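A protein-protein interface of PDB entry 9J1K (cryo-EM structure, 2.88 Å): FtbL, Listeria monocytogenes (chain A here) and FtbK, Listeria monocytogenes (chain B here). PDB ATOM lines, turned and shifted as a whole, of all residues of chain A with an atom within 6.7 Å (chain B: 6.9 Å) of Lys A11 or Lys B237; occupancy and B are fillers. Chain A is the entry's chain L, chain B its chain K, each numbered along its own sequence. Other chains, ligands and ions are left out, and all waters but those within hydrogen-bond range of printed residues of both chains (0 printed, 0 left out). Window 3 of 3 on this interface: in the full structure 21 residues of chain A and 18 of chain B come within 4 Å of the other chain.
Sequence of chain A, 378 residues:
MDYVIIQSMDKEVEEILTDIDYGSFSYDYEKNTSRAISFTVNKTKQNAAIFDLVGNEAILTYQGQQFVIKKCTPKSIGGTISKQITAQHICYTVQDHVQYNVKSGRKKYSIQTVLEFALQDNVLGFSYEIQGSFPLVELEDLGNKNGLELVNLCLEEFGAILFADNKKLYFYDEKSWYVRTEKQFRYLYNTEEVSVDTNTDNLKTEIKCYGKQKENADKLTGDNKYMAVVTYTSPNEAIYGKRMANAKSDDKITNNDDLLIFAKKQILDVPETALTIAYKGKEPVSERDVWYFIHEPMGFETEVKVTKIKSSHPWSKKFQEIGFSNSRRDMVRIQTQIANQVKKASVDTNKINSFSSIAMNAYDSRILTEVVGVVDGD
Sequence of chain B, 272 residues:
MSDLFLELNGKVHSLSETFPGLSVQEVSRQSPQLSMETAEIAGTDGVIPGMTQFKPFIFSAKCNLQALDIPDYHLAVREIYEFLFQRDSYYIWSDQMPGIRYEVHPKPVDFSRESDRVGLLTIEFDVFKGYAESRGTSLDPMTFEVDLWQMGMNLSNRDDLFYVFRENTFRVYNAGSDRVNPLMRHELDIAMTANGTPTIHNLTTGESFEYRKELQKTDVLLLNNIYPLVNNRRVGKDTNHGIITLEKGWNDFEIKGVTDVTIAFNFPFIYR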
ATOM      1  N   GLN A   7      33.201  11.133  18.316  1.00  0.00           N
ATOM      2  CA  GLN A   7      32.444  10.400  17.314  1.00  0.00           C
ATOM      3  C   GLN A   7      32.713   8.916  17.502  1.00  0.00           C
ATOM      4  O   GLN A   7      33.875   8.496  17.582  1.00  0.00           O
ATOM      5  CB  GLN A   7      32.826  10.844  15.900  1.00  0.00           C
ATOM      6  CG  GLN A   7      32.008  10.189  14.803  1.00  0.00           C
ATOM      7  CD  GLN A   7      32.785  10.043  13.512  1.00  0.00           C
ATOM      8  OE1 GLN A   7      33.755   9.290  13.441  1.00  0.00           O
ATOM      9  NE2 GLN A   7      32.363  10.766  12.483  1.00  0.00           N
ATOM     10  N   SER A   8      31.642   8.130  17.564  1.00  0.00           N
ATOM     11  CA  SER A   8      31.740   6.723  17.913  1.00  0.00           C
ATOM     12  C   SER A   8      32.434   5.932  16.805  1.00  0.00           C
ATOM     13  O   SER A   8      32.707   6.436  15.712  1.00  0.00           O
ATOM     14  CB  SER A   8      30.355   6.144  18.186  1.00  0.00           C
ATOM     15  OG  SER A   8      29.885   6.529  19.466  1.00  0.00           O
ATOM     16  N   MET A   9      32.723   4.666  17.114  1.00  0.00           N
ATOM     17  CA  MET A   9      33.384   3.794  16.148  1.00  0.00           C
ATOM     18  C   MET A   9      32.524   3.588  14.909  1.00  0.00           C
ATOM     19  O   MET A   9      33.033   3.596  13.782  1.00  0.00           O
ATOM     20  CB  MET A   9      33.714   2.453  16.801  1.00  0.00           C
ATOM     21  CG  MET A   9      34.627   1.567  15.976  1.00  0.00           C
ATOM     22  SD  MET A   9      34.656  -0.126  16.589  1.00  0.00           S
ATOM     23  CE  MET A   9      34.666   0.153  18.356  1.00  0.00           C
ATOM     24  N   ASP A  10      31.220   3.402  15.095  1.00  0.00           N
ATOM     25  CA  ASP A  10      30.303   3.224  13.979  1.00  0.00           C
ATOM     26  C   ASP A  10      29.814   4.543  13.399  1.00  0.00           C
ATOM     27  O   ASP A  10      29.008   4.526  12.461  1.00  0.00           O
ATOM     28  CB  ASP A  10      29.105   2.375  14.414  1.00  0.00           C
ATOM     29  CG  ASP A  10      28.394   2.947  15.622  1.00  0.00           C
ATOM     30  OD1 ASP A  10      28.908   3.918  16.214  1.00  0.00           O
ATOM     31  OD2 ASP A  10      27.318   2.423  15.982  1.00  0.00           O
ATOM     32  N   LYS A  11      30.273   5.676  13.935  1.00  0.00           N
ATOM     33  CA  LYS A  11      29.915   7.012  13.461  1.00  0.00           C
ATOM     34  C   LYS A  11      28.414   7.272  13.530  1.00  0.00           C
ATOM     35  O   LYS A  11      27.896   8.130  12.811  1.00  0.00           O
ATOM     36  CB  LYS A  11      30.427   7.254  12.035  1.00  0.00           C
ATOM     37  CG  LYS A  11      31.809   6.678  11.765  1.00  0.00           C
ATOM     38  CD  LYS A  11      32.255   6.947  10.340  1.00  0.00           C
ATOM     39  CE  LYS A  11      33.738   7.272  10.282  1.00  0.00           C
ATOM     40  NZ  LYS A  11      34.573   6.044  10.373  1.00  0.00           N
ATOM     41  N   GLU A  12      27.703   6.541  14.389  1.00  0.00           N
ATOM     42  CA  GLU A  12      26.262   6.735  14.515  1.00  0.00           C
ATOM     43  C   GLU A  12      25.927   7.998  15.295  1.00  0.00           C
ATOM     44  O   GLU A  12      24.973   8.704  14.954  1.00  0.00           O
ATOM     45  CB  GLU A  12      25.626   5.516  15.181  1.00  0.00           C
ATOM     46  CG  GLU A  12      25.336   4.368  14.230  1.00  0.00           C
ATOM     47  CD  GLU A  12      24.528   4.803  13.023  1.00  0.00           C
ATOM     48  OE1 GLU A  12      23.286   4.871  13.132  1.00  0.00           O
ATOM     49  OE2 GLU A  12      25.134   5.072  11.964  1.00  0.00           O
ATOM     50  N   VAL A  13      26.693   8.298  16.341  1.00  0.00           N
ATOM     51  CA  VAL A  13      26.413   9.419  17.228  1.00  0.00           C
ATOM     52  C   VAL A  13      27.684  10.239  17.401  1.00  0.00           C
ATOM     53  O   VAL A  13      28.760   9.684  17.646  1.00  0.00           O
ATOM     54  CB  VAL A  13      25.878   8.939  18.591  1.00  0.00           C
ATOM     55  CG1 VAL A  13      26.720   7.790  19.114  1.00  0.00           C
ATOM     56  CG2 VAL A  13      25.852  10.084  19.591  1.00  0.00           C
ATOM     57  N   GLU A  14      27.559  11.557  17.258  1.00  0.00           N
ATOM     58  CA  GLU A  14      28.668  12.484  17.444  1.00  0.00           C
ATOM     59  C   GLU A  14      28.222  13.570  18.410  1.00  0.00           C
ATOM     60  O   GLU A  14      27.220  14.249  18.162  1.00  0.00           O
ATOM     61  CB  GLU A  14      29.108  13.087  16.108  1.00  0.00           C
ATOM     62  CG  GLU A  14      30.137  14.192  16.228  1.00  0.00           C
ATOM     63  CD  GLU A  14      30.873  14.441  14.926  1.00  0.00           C
ATOM     64  OE1 GLU A  14      30.316  15.135  14.051  1.00  0.00           O
ATOM     65  OE2 GLU A  14      32.007  13.942  14.779  1.00  0.00           O
ATOM     66  N   GLU A  15      28.961  13.735  19.504  1.00  0.00           N
ATOM     67  CA  GLU A  15      28.576  14.662  20.563  1.00  0.00           C
ATOM     68  C   GLU A  15      29.823  15.391  21.049  1.00  0.00           C
ATOM     69  O   GLU A  15      30.896  15.301  20.447  1.00  0.00           O
ATOM     70  CB  GLU A  15      27.865  13.921  21.702  1.00  0.00           C
ATOM     71  CG  GLU A  15      26.469  13.434  21.357  1.00  0.00           C
ATOM     72  CD  GLU A  15      25.554  14.556  20.909  1.00  0.00           C
ATOM     73  OE1 GLU A  15      25.599  15.642  21.524  1.00  0.00           O
ATOM     74  OE2 GLU A  15      24.790  14.352  19.943  1.00  0.00           O
ATOM     75  N   ILE A  59      36.808   8.493  17.413  1.00  0.00           N
ATOM     76  CA  ILE A  59      37.431   9.639  16.762  1.00  0.00           C
ATOM     77  C   ILE A  59      37.192  10.876  17.615  1.00  0.00           C
ATOM     78  O   ILE A  59      36.064  11.132  18.047  1.00  0.00           O
ATOM     79  CB  ILE A  59      36.896   9.845  15.334  1.00  0.00           C
ATOM     80  CG1 ILE A  59      36.995   8.540  14.540  1.00  0.00           C
ATOM     81  CG2 ILE A  59      37.645  10.975  14.642  1.00  0.00           C
ATOM     82  CD1 ILE A  59      38.255   8.413  13.711  1.00  0.00           C
ATOM     83  N   LYS A 167      43.180  13.693   6.769  1.00  0.00           N
ATOM     84  CA  LYS A 167      43.570  12.581   5.914  1.00  0.00           C
ATOM     85  C   LYS A 167      44.325  13.021   4.667  1.00  0.00           C
ATOM     86  O   LYS A 167      44.532  12.206   3.763  1.00  0.00           O
ATOM     87  CB  LYS A 167      42.337  11.767   5.517  1.00  0.00           C
ATOM     88  CG  LYS A 167      42.094  10.554   6.396  1.00  0.00           C
ATOM     89  CD  LYS A 167      40.692  10.006   6.208  1.00  0.00           C
ATOM     90  CE  LYS A 167      40.504   8.709   6.973  1.00  0.00           C
ATOM     91  NZ  LYS A 167      39.105   8.212   6.878  1.00  0.00           N
ATOM     92  N   ARG B 212      21.647  21.994  10.582  1.00  0.00           N
ATOM     93  CA  ARG B 212      21.756  21.889   9.131  1.00  0.00           C
ATOM     94  C   ARG B 212      20.676  20.994   8.530  1.00  0.00           C
ATOM     95  O   ARG B 212      20.924  20.250   7.580  1.00  0.00           O
ATOM     96  CB  ARG B 212      23.140  21.384   8.739  1.00  0.00           C
ATOM     97  CG  ARG B 212      24.263  21.979   9.568  1.00  0.00           C
ATOM     98  CD  ARG B 212      25.314  22.635   8.692  1.00  0.00           C
ATOM     99  NE  ARG B 212      26.459  23.095   9.468  1.00  0.00           N
ATOM    100  CZ  ARG B 212      27.426  22.306   9.918  1.00  0.00           C
ATOM    101  NH1 ARG B 212      27.418  21.003   9.688  1.00  0.00           N
ATOM    102  NH2 ARG B 212      28.424  22.837  10.616  1.00  0.00           N
ATOM    103  N   PRO B 228      22.121  18.801  21.887  1.00  0.00           N
ATOM    104  CA  PRO B 228      20.975  19.198  21.064  1.00  0.00           C
ATOM    105  C   PRO B 228      20.172  17.991  20.607  1.00  0.00           C
ATOM    106  O   PRO B 228      20.717  16.973  20.174  1.00  0.00           O
ATOM    107  CB  PRO B 228      21.642  19.900  19.875  1.00  0.00           C
ATOM    108  CG  PRO B 228      22.970  19.210  19.737  1.00  0.00           C
ATOM    109  CD  PRO B 228      23.345  18.633  21.085  1.00  0.00           C
ATOM    110  N   ARG B 234      19.040  12.504  19.629  1.00  0.00           N
ATOM    111  CA  ARG B 234      20.319  13.188  19.488  1.00  0.00           C
ATOM    112  C   ARG B 234      20.637  13.433  18.019  1.00  0.00           C
ATOM    113  O   ARG B 234      20.631  12.504  17.207  1.00  0.00           O
ATOM    114  CB  ARG B 234      21.428  12.367  20.142  1.00  0.00           C
ATOM    115  CG  ARG B 234      21.184  12.071  21.609  1.00  0.00           C
ATOM    116  CD  ARG B 234      22.479  11.790  22.349  1.00  0.00           C
ATOM    117  NE  ARG B 234      22.234  11.411  23.734  1.00  0.00           N
ATOM    118  CZ  ARG B 234      21.912  12.264  24.698  1.00  0.00           C
ATOM    119  NH1 ARG B 234      21.818  13.563  24.468  1.00  0.00           N
ATOM    120  NH2 ARG B 234      21.680  11.801  25.922  1.00  0.00           N
ATOM    121  N   VAL B 235      20.915  14.690  17.681  1.00  0.00           N
ATOM    122  CA  VAL B 235      21.218  15.078  16.308  1.00  0.00           C
ATOM    123  C   VAL B 235      22.520  15.864  16.263  1.00  0.00           C
ATOM    124  O   VAL B 235      22.702  16.731  15.403  1.00  0.00           O
ATOM    125  CB  VAL B 235      20.066  15.892  15.693  1.00  0.00           C
ATOM    126  CG1 VAL B 235      18.893  14.983  15.386  1.00  0.00           C
ATOM    127  CG2 VAL B 235      19.651  17.009  16.635  1.00  0.00           C
ATOM    128  N   GLY B 236      23.432  15.570  17.192  1.00  0.00           N
ATOM    129  CA  GLY B 236      24.682  16.310  17.255  1.00  0.00           C
ATOM    130  C   GLY B 236      25.509  16.214  15.989  1.00  0.00           C
ATOM    131  O   GLY B 236      26.304  17.110  15.695  1.00  0.00           O
ATOM    132  N   LYS B 237      25.341  15.133  15.224  1.00  0.00           N
ATOM    133  CA  LYS B 237      26.104  14.972  13.992  1.00  0.00           C
ATOM    134  C   LYS B 237      25.700  15.991  12.934  1.00  0.00           C
ATOM    135  O   LYS B 237      26.499  16.310  12.047  1.00  0.00           O
ATOM    136  CB  LYS B 237      25.925  13.557  13.446  1.00  0.00           C
ATOM    137  CG  LYS B 237      24.491  13.062  13.488  1.00  0.00           C
ATOM    138  CD  LYS B 237      24.427  11.546  13.517  1.00  0.00           C
ATOM    139  CE  LYS B 237      25.136  10.941  12.318  1.00  0.00           C
ATOM    140  NZ  LYS B 237      24.707  11.574  11.041  1.00  0.00           N
ATOM    141  N   ASP B 238      24.475  16.510  13.006  1.00  0.00           N
ATOM    142  CA  ASP B 238      23.940  17.407  11.992  1.00  0.00           C
ATOM    143  C   ASP B 238      24.044  18.875  12.388  1.00  0.00           C
ATOM    144  O   ASP B 238      23.417  19.727  11.752  1.00  0.00           O
ATOM    145  CB  ASP B 238      22.486  17.047  11.687  1.00  0.00           C
ATOM    146  CG  ASP B 238      22.263  15.553  11.597  1.00  0.00           C
ATOM    147  OD1 ASP B 238      22.960  14.895  10.796  1.00  0.00           O
ATOM    148  OD2 ASP B 238      21.394  15.035  12.328  1.00  0.00           O
ATOM    149  N   THR B 239      24.815  19.185  13.421  1.00  0.00           N
ATOM    150  CA  THR B 239      24.997  20.553  13.886  1.00  0.00           C
ATOM    151  C   THR B 239      26.456  20.964  13.720  1.00  0.00           C
ATOM    152  O   THR B 239      27.307  20.174  13.307  1.00  0.00           O
ATOM    153  CB  THR B 239      24.562  20.698  15.348  1.00  0.00           C
ATOM    154  OG1 THR B 239      25.574  20.156  16.204  1.00  0.00           O
ATOM    155  CG2 THR B 239      23.254  19.968  15.593  1.00  0.00           C
ATOM    156  N   ASN B 240      26.736  22.221  14.049  1.00  0.00           N
ATOM    157  CA  ASN B 240      28.097  22.738  14.056  1.00  0.00           C
ATOM    158  C   ASN B 240      28.786  22.535  15.396  1.00  0.00           C
ATOM    159  O   ASN B 240      29.923  22.989  15.566  1.00  0.00           O
ATOM    160  CB  ASN B 240      28.102  24.225  13.696  1.00  0.00           C
ATOM    161  CG  ASN B 240      27.467  25.083  14.768  1.00  0.00           C
ATOM    162  OD1 ASN B 240      26.431  24.729  15.330  1.00  0.00           O
ATOM    163  ND2 ASN B 240      28.088  26.219  15.062  1.00  0.00           N
ATOM    164  N   HIS B 241      28.118  21.884  16.346  1.00  0.00           N
ATOM    165  CA  HIS B 241      28.628  21.583  17.680  1.00  0.00           C
ATOM    166  C   HIS B 241      28.908  22.832  18.504  1.00  0.00           C
ATOM    167  O   HIS B 241      29.530  22.739  19.568  1.00  0.00           O
ATOM    168  CB  HIS B 241      29.883  20.706  17.616  1.00  0.00           C
ATOM    169  CG  HIS B 241      29.623  19.327  17.103  1.00  0.00           C
ATOM    170  ND1 HIS B 241      30.043  18.903  15.861  1.00  0.00           N
ATOM    171  CD2 HIS B 241      28.980  18.275  17.662  1.00  0.00           C
ATOM    172  CE1 HIS B 241      29.672  17.648  15.678  1.00  0.00           C
ATOM    173  NE2 HIS B 241      29.025  17.244  16.756  1.00  0.00           N
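OE2 of Glu A15 sits at hydrogen-bond distance from N of Gly B236, at 3.3 Å.
The backbone carbonyl oxygen of Pro B228 is in hydrogen-bond range of the backbone NH of Val B235, at 3.4 Å.
The backbone carbonyl oxygen (O) of Gly B236 sits at hydrogen-bond distance from the side-chain hydroxyl (OG1) of Thr B239 (3.2 Å).
The backbone carbonyl oxygen (O) of Gly B236 is in hydrogen-bond range of a ring nitrogen (NE2) of His B241.
OD1 of Asp B238 lies within salt-bridge range of NZ of Lys B237 (3.8 Å).
The side-chain hydroxyl (OG1) of Thr B239 sits at hydrogen-bond distance from the backbone NH (N) of His B241.
The side-chain carboxylate of Asp A10 sits close to the backbone NH of Glu A12, 3.4 Å away.
O of Lys A11 touches CE of Lys B237 (3.97 Å).
CD of Lys B237 touches O of Glu A12, 3.2 Å away.
O of Glu A14 touches C of Gly B236 (3.4 Å).
Glu A14 touches Lys B237.
Glu A14 touches His B241 (OE1 to CE1, 3.1 Å).
Glu A15 touches Pro B228.
Arg B234 touches Glu A15.
Lys A11 touches one residue of chain B.
Of chain A, only Lys A11, Glu A12 and Glu A14 come within 4 Å of Lys B237.
Printed residues of chain B within 4 Å of Glu A15: Pro B228 (3.8 Å), Arg B234 (3.9 Å) and Gly B236 (3.3 Å).
Of the printed residues of chain A, Arg B234 touches Glu A15 (3.9 Å).
Of the printed residues of chain B, Glu A14 touches Gly B236, Lys B237 and His B241.
Gln A7 touches none of the printed residues of chain B.
Val B235 touches none of the printed residues of chain A.
The nearest printed residue of chain B that does not touch Lys A11 is Asp B238 (8.6 Å).
Among the printed residues, no Asp or Glu carboxylate lies within 4 Å of a Lys or Arg side-chain nitrogen of the other chain.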
